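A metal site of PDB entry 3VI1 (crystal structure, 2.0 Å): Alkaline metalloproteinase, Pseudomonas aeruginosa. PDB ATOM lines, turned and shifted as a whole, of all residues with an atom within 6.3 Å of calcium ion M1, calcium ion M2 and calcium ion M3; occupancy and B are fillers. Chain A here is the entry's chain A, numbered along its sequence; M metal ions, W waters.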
ATOM      1  N   GLY A 333      28.829  13.270  -4.042  1.00  0.00           N
ATOM      2  CA  GLY A 333      29.835  13.526  -5.071  1.00  0.00           C
ATOM      3  C   GLY A 333      31.192  13.864  -4.467  1.00  0.00           C
ATOM      4  O   GLY A 333      31.313  14.007  -3.250  1.00  0.00           O
ATOM      5  N   GLY A 334      32.196  13.984  -5.319  1.00  0.00           N
ATOM      6  CA  GLY A 334      33.546  14.342  -4.875  1.00  0.00           C
ATOM      7  C   GLY A 334      33.824  15.830  -5.014  1.00  0.00           C
ATOM      8  O   GLY A 334      32.903  16.634  -5.094  1.00  0.00           O
ATOM      9  N   SER A 335      35.109  16.183  -5.051  1.00  0.00           N
ATOM     10  CA  SER A 335      35.534  17.582  -5.144  1.00  0.00           C
ATOM     11  C   SER A 335      35.420  18.171  -6.559  1.00  0.00           C
ATOM     12  O   SER A 335      35.526  19.384  -6.740  1.00  0.00           O
ATOM     13  CB  SER A 335      36.951  17.762  -4.601  1.00  0.00           C
ATOM     14  OG  SER A 335      37.874  16.945  -5.299  1.00  0.00           O
ATOM     15  N   GLY A 336      35.197  17.304  -7.551  1.00  0.00           N
ATOM     16  CA  GLY A 336      35.020  17.733  -8.932  1.00  0.00           C
ATOM     17  C   GLY A 336      33.619  18.217  -9.221  1.00  0.00           C
ATOM     18  O   GLY A 336      32.729  18.141  -8.362  1.00  0.00           O
ATOM     19  N   SER A 337      33.414  18.732 -10.433  1.00  0.00           N
ATOM     20  CA  SER A 337      32.095  19.180 -10.865  1.00  0.00           C
ATOM     21  C   SER A 337      31.228  17.992 -11.266  1.00  0.00           C
ATOM     22  O   SER A 337      31.406  17.409 -12.326  1.00  0.00           O
ATOM     23  CB  SER A 337      32.227  20.186 -12.020  1.00  0.00           C
ATOM     24  OG  SER A 337      32.817  21.385 -11.572  1.00  0.00           O
ATOM     25  N   ASP A 338      30.290  17.643 -10.386  1.00  0.00           N
ATOM     26  CA  ASP A 338      29.541  16.396 -10.515  1.00  0.00           C
ATOM     27  C   ASP A 338      28.107  16.575 -10.994  1.00  0.00           C
ATOM     28  O   ASP A 338      27.521  17.656 -10.886  1.00  0.00           O
ATOM     29  CB  ASP A 338      29.531  15.635  -9.182  1.00  0.00           C
ATOM     30  CG  ASP A 338      30.929  15.368  -8.652  1.00  0.00           C
ATOM     31  OD1 ASP A 338      31.795  14.913  -9.433  1.00  0.00           O
ATOM     32  OD2 ASP A 338      31.154  15.613  -7.442  1.00  0.00           O
ATOM     33  N   LEU A 340      24.496  14.742 -10.235  1.00  0.00           N
ATOM     34  CA  LEU A 340      23.804  13.827  -9.335  1.00  0.00           C
ATOM     35  C   LEU A 340      22.316  13.727  -9.655  1.00  0.00           C
ATOM     36  O   LEU A 340      21.559  14.687  -9.454  1.00  0.00           O
ATOM     37  CB  LEU A 340      24.012  14.236  -7.861  1.00  0.00           C
ATOM     38  CG  LEU A 340      25.293  13.789  -7.161  1.00  0.00           C
ATOM     39  CD1 LEU A 340      26.457  14.710  -7.494  1.00  0.00           C
ATOM     40  CD2 LEU A 340      25.076  13.744  -5.658  1.00  0.00           C
ATOM     41  N   LYS A 350      24.341  15.134  -2.098  1.00  0.00           N
ATOM     42  CA  LYS A 350      25.394  16.054  -1.678  1.00  0.00           C
ATOM     43  C   LYS A 350      26.453  16.203  -2.767  1.00  0.00           C
ATOM     44  O   LYS A 350      27.090  15.225  -3.172  1.00  0.00           O
ATOM     45  CB  LYS A 350      26.018  15.590  -0.352  1.00  0.00           C
ATOM     46  CG  LYS A 350      25.055  15.636   0.824  1.00  0.00           C
ATOM     47  CD  LYS A 350      25.740  15.346   2.143  1.00  0.00           C
ATOM     48  CE  LYS A 350      24.764  15.512   3.296  1.00  0.00           C
ATOM     49  NZ  LYS A 350      25.373  15.178   4.612  1.00  0.00           N
ATOM     50  N   GLY A 351      26.619  17.427  -3.247  1.00  0.00           N
ATOM     51  CA  GLY A 351      27.544  17.715  -4.339  1.00  0.00           C
ATOM     52  C   GLY A 351      28.991  17.848  -3.905  1.00  0.00           C
ATOM     53  O   GLY A 351      29.898  17.471  -4.658  1.00  0.00           O
ATOM     54  N   GLY A 352      29.215  18.384  -2.716  1.00  0.00           N
ATOM     55  CA  GLY A 352      30.572  18.656  -2.224  1.00  0.00           C
ATOM     56  C   GLY A 352      31.169  19.862  -2.924  1.00  0.00           C
ATOM     57  O   GLY A 352      30.451  20.754  -3.360  1.00  0.00           O
ATOM     58  N   ALA A 353      32.495  19.871  -3.044  1.00  0.00           N
ATOM     59  CA  ALA A 353      33.203  20.941  -3.746  1.00  0.00           C
ATOM     60  C   ALA A 353      32.944  20.889  -5.261  1.00  0.00           C
ATOM     61  O   ALA A 353      32.464  19.881  -5.778  1.00  0.00           O
ATOM     62  CB  ALA A 353      34.704  20.872  -3.460  1.00  0.00           C
ATOM     63  N   GLY A 354      33.270  21.988  -5.948  1.00  0.00           N
ATOM     64  CA  GLY A 354      33.062  22.075  -7.392  1.00  0.00           C
ATOM     65  C   GLY A 354      31.652  22.505  -7.758  1.00  0.00           C
ATOM     66  O   GLY A 354      30.787  22.636  -6.895  1.00  0.00           O
ATOM     67  N   ASN A 355      31.426  22.710  -9.061  1.00  0.00           N
ATOM     68  CA  ASN A 355      30.141  23.169  -9.569  1.00  0.00           C
ATOM     69  C   ASN A 355      29.229  22.010  -9.964  1.00  0.00           C
ATOM     70  O   ASN A 355      29.356  21.441 -11.051  1.00  0.00           O
ATOM     71  CB  ASN A 355      30.348  24.131 -10.744  1.00  0.00           C
ATOM     72  CG  ASN A 355      31.125  25.376 -10.359  1.00  0.00           C
ATOM     73  OD1 ASN A 355      31.044  25.849  -9.218  1.00  0.00           O
ATOM     74  ND2 ASN A 355      31.879  25.915 -11.303  1.00  0.00           N
ATOM     75  N   ASP A 356      28.293  21.683  -9.080  1.00  0.00           N
ATOM     76  CA  ASP A 356      27.486  20.480  -9.225  1.00  0.00           C
ATOM     77  C   ASP A 356      26.076  20.746  -9.740  1.00  0.00           C
ATOM     78  O   ASP A 356      25.487  21.794  -9.470  1.00  0.00           O
ATOM     79  CB  ASP A 356      27.411  19.710  -7.908  1.00  0.00           C
ATOM     80  CG  ASP A 356      28.776  19.452  -7.312  1.00  0.00           C
ATOM     81  OD1 ASP A 356      29.560  18.690  -7.923  1.00  0.00           O
ATOM     82  OD2 ASP A 356      29.075  19.996  -6.229  1.00  0.00           O
ATOM     83  N   TRP A 368      21.962  19.150  -1.042  1.00  0.00           N
ATOM     84  CA  TRP A 368      23.118  19.906  -0.570  1.00  0.00           C
ATOM     85  C   TRP A 368      24.046  20.173  -1.752  1.00  0.00           C
ATOM     86  O   TRP A 368      24.515  19.253  -2.404  1.00  0.00           O
ATOM     87  CB  TRP A 368      23.878  19.115   0.508  1.00  0.00           C
ATOM     88  CG  TRP A 368      23.020  18.634   1.659  1.00  0.00           C
ATOM     89  CD1 TRP A 368      22.119  17.608   1.638  1.00  0.00           C
ATOM     90  CD2 TRP A 368      23.027  19.136   3.004  1.00  0.00           C
ATOM     91  NE1 TRP A 368      21.541  17.458   2.873  1.00  0.00           N
ATOM     92  CE2 TRP A 368      22.081  18.378   3.728  1.00  0.00           C
ATOM     93  CE3 TRP A 368      23.723  20.161   3.662  1.00  0.00           C
ATOM     94  CZ2 TRP A 368      21.818  18.608   5.095  1.00  0.00           C
ATOM     95  CZ3 TRP A 368      23.466  20.389   5.008  1.00  0.00           C
ATOM     96  CH2 TRP A 368      22.524  19.608   5.706  1.00  0.00           C
ATOM     97  N   GLY A 369      24.279  21.454  -2.015  1.00  0.00           N
ATOM     98  CA  GLY A 369      25.175  21.851  -3.092  1.00  0.00           C
ATOM     99  C   GLY A 369      26.636  21.785  -2.696  1.00  0.00           C
ATOM    100  O   GLY A 369      27.491  21.367  -3.482  1.00  0.00           O
ATOM    101  N   GLY A 370      26.929  22.169  -1.453  1.00  0.00           N
ATOM    102  CA  GLY A 370      28.299  22.305  -0.979  1.00  0.00           C
ATOM    103  C   GLY A 370      28.890  23.620  -1.465  1.00  0.00           C
ATOM    104  O   GLY A 370      28.141  24.545  -1.818  1.00  0.00           O
ATOM    105  N   ALA A 371      30.212  23.701  -1.502  1.00  0.00           N
ATOM    106  CA  ALA A 371      30.901  24.882  -2.026  1.00  0.00           C
ATOM    107  C   ALA A 371      30.762  24.959  -3.545  1.00  0.00           C
ATOM    108  O   ALA A 371      30.481  23.949  -4.198  1.00  0.00           O
ATOM    109  CB  ALA A 371      32.354  24.878  -1.616  1.00  0.00           C
ATOM    110  N   GLY A 372      30.975  26.146  -4.094  1.00  0.00           N
ATOM    111  CA  GLY A 372      30.899  26.365  -5.545  1.00  0.00           C
ATOM    112  C   GLY A 372      29.495  26.698  -6.034  1.00  0.00           C
ATOM    113  O   GLY A 372      28.533  26.663  -5.269  1.00  0.00           O
ATOM    114  N   ALA A 373      29.401  27.026  -7.320  1.00  0.00           N
ATOM    115  CA  ALA A 373      28.130  27.379  -7.956  1.00  0.00           C
ATOM    116  C   ALA A 373      27.365  26.134  -8.371  1.00  0.00           C
ATOM    117  O   ALA A 373      27.693  25.488  -9.367  1.00  0.00           O
ATOM    118  CB  ALA A 373      28.386  28.289  -9.163  1.00  0.00           C
ATOM    119  N   ASP A 374      26.328  25.805  -7.609  1.00  0.00           N
ATOM    120  CA  ASP A 374      25.553  24.591  -7.833  1.00  0.00           C
ATOM    121  C   ASP A 374      24.185  24.879  -8.440  1.00  0.00           C
ATOM    122  O   ASP A 374      23.595  25.925  -8.184  1.00  0.00           O
ATOM    123  CB  ASP A 374      25.415  23.801  -6.530  1.00  0.00           C
ATOM    124  CG  ASP A 374      26.746  23.463  -5.907  1.00  0.00           C
ATOM    125  OD1 ASP A 374      27.488  22.633  -6.469  1.00  0.00           O
ATOM    126  OD2 ASP A 374      27.066  24.032  -4.843  1.00  0.00           O
ATOM    127  N   PHE A 376      20.280  23.402  -9.037  1.00  0.00           N
ATOM    128  CA  PHE A 376      19.224  22.488  -8.641  1.00  0.00           C
ATOM    129  C   PHE A 376      18.150  22.486  -9.727  1.00  0.00           C
ATOM    130  O   PHE A 376      17.433  23.474  -9.905  1.00  0.00           O
ATOM    131  CB  PHE A 376      18.662  22.873  -7.268  1.00  0.00           C
ATOM    132  CG  PHE A 376      19.719  23.035  -6.204  1.00  0.00           C
ATOM    133  CD1 PHE A 376      20.231  24.298  -5.904  1.00  0.00           C
ATOM    134  CD2 PHE A 376      20.222  21.922  -5.528  1.00  0.00           C
ATOM    135  CE1 PHE A 376      21.216  24.449  -4.926  1.00  0.00           C
ATOM    136  CE2 PHE A 376      21.206  22.073  -4.550  1.00  0.00           C
ATOM    137  CZ  PHE A 376      21.705  23.332  -4.248  1.00  0.00           C
ATOM    138  N   ASP A 394      21.625  24.157   1.782  1.00  0.00           N
ATOM    139  CA  ASP A 394      22.752  25.090   1.887  1.00  0.00           C
ATOM    140  C   ASP A 394      22.801  26.105   0.743  1.00  0.00           C
ATOM    141  O   ASP A 394      23.875  26.424   0.231  1.00  0.00           O
ATOM    142  CB  ASP A 394      24.088  24.328   2.026  1.00  0.00           C
ATOM    143  CG  ASP A 394      24.358  23.390   0.846  1.00  0.00           C
ATOM    144  OD1 ASP A 394      23.560  23.347  -0.110  1.00  0.00           O
ATOM    145  OD2 ASP A 394      25.399  22.698   0.881  1.00  0.00           O
ATOM    146  N   VAL A 396      23.065  29.328  -1.353  1.00  0.00           N
ATOM    147  CA  VAL A 396      23.741  30.613  -1.253  1.00  0.00           C
ATOM    148  C   VAL A 396      23.301  31.495  -2.423  1.00  0.00           C
ATOM    149  O   VAL A 396      23.493  31.144  -3.589  1.00  0.00           O
ATOM    150  CB  VAL A 396      25.292  30.458  -1.272  1.00  0.00           C
ATOM    151  CG1 VAL A 396      25.972  31.821  -1.148  1.00  0.00           C
ATOM    152  CG2 VAL A 396      25.756  29.524  -0.154  1.00  0.00           C
ATOM    153  N   GLN A 399      25.237  32.675  -6.024  1.00  0.00           N
ATOM    154  CA  GLN A 399      26.184  31.618  -6.353  1.00  0.00           C
ATOM    155  C   GLN A 399      25.450  30.380  -6.870  1.00  0.00           C
ATOM    156  O   GLN A 399      25.750  29.880  -7.965  1.00  0.00           O
ATOM    157  CB  GLN A 399      27.046  31.259  -5.143  1.00  0.00           C
ATOM    158  CG  GLN A 399      28.243  30.370  -5.456  1.00  0.00           C
ATOM    159  CD  GLN A 399      29.011  29.937  -4.215  1.00  0.00           C
ATOM    160  OE1 GLN A 399      28.419  29.654  -3.175  1.00  0.00           O
ATOM    161  NE2 GLN A 399      30.328  29.870  -4.338  1.00  0.00           N
ATOM    162  N   ASP A 400      24.487  29.895  -6.091  1.00  0.00           N
ATOM    163  CA  ASP A 400      23.677  28.746  -6.480  1.00  0.00           C
ATOM    164  C   ASP A 400      22.532  29.154  -7.384  1.00  0.00           C
ATOM    165  O   ASP A 400      22.164  30.340  -7.449  1.00  0.00           O
ATOM    166  CB  ASP A 400      23.136  28.031  -5.239  1.00  0.00           C
ATOM    167  CG  ASP A 400      24.229  27.446  -4.371  1.00  0.00           C
ATOM    168  OD1 ASP A 400      25.243  26.946  -4.920  1.00  0.00           O
ATOM    169  OD2 ASP A 400      24.075  27.470  -3.132  1.00  0.00           O
HETATM  170 CA    CA M   1      27.051  25.896  -3.454  1.00  0.00          CA
HETATM  171 CA    CA M   2      29.335  22.034  -4.999  1.00  0.00          CA
HETATM  172 CA    CA M   3      31.350  17.878  -6.433  1.00  0.00          CA
HETATM  173  O   HOH W   1      27.917  27.379  -1.764  1.00  0.00           O
HETATM  174  O   HOH W   2      25.026  25.116  -2.267  1.00  0.00           O
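The backbone NH (N) of Gly 370 is in hydrogen-bond range of the side-chain carboxylate (OD2) of Asp 394, at 2.8 Å. N of Gly 351 lies within hydrogen-bond range of O of Trp 368, 2.9 Å away. The backbone NH (N) of Val 396 sits at hydrogen-bond distance from the side-chain carboxylate (OD2) of Asp 400, 2.8 Å away. The backbone NH (N) of Gly 369 lies within hydrogen-bond range of the side-chain carboxylate (OD1) of Asp 394, at 2.8 Å.
Five residues have an atom within 4 Å of calcium ion M1: Gly 370, Ala 371, Gly 372, Asp 374 and Asp 400.
Eight residues have an atom within 4 Å of calcium ion M2: Gly 352, Ala 353, Gly 354, Asp 356, Gly 369, Gly 370, Ala 371 and Asp 374. The nearest printed residue that does not touch calcium ion M2 is Gly 351 (4.3 Å).
The nearest printed residue that does not touch calcium ion M3 is Gly 352 (4.04 Å).
The side-chain carboxylate (OD2) of Asp 374 is bound to calcium ion M1 (2.3 Å). Calcium ion M1 is bound by O of Gly 370, at 2.4 Å. Water W1 binds calcium ion M1, 2.4 Å away. The backbone carbonyl oxygen (O) of Gly 372 is bound to calcium ion M1, 2.5 Å away. Water W2 is bound to calcium ion M1, at 2.5 Å. OD1 of Asp 400 binds calcium ion M1 (2.6 Å). Calcium ion M1 has six donor atoms within binding distance.
Calcium ion M2 is bound by O of Gly 352 (2.4 Å), O of Ala 371 (2.4 Å), OD2 of Asp 356 (2.4 Å), OD1 of Asp 374 (2.4 Å), O of Gly 354 (2.5 Å) and O of Gly 369 (2.5 Å). Slightly farther from calcium ion M2 lies OD2 of Asp 374 (3.0 Å).
Calcium ion M3 is bound by O of Gly 351 (2.3 Å), O of Ala 353 (2.4 Å), O of Gly 336 (2.4 Å), O of Gly 334 (2.4 Å), OD1 of Asp 356 (2.5 Å) and OD2 of Asp 338 (2.5 Å). Calcium ion M3 has six donor atoms within binding distance. Slightly farther from calcium ion M3 lies the side-chain carboxylate (OD2) of Asp 356 (3.1 Å).
Water W2 lies within hydrogen-bond range of OD2 of Asp 400 (2.7 Å) and O of Asp 394 (3.0 Å).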
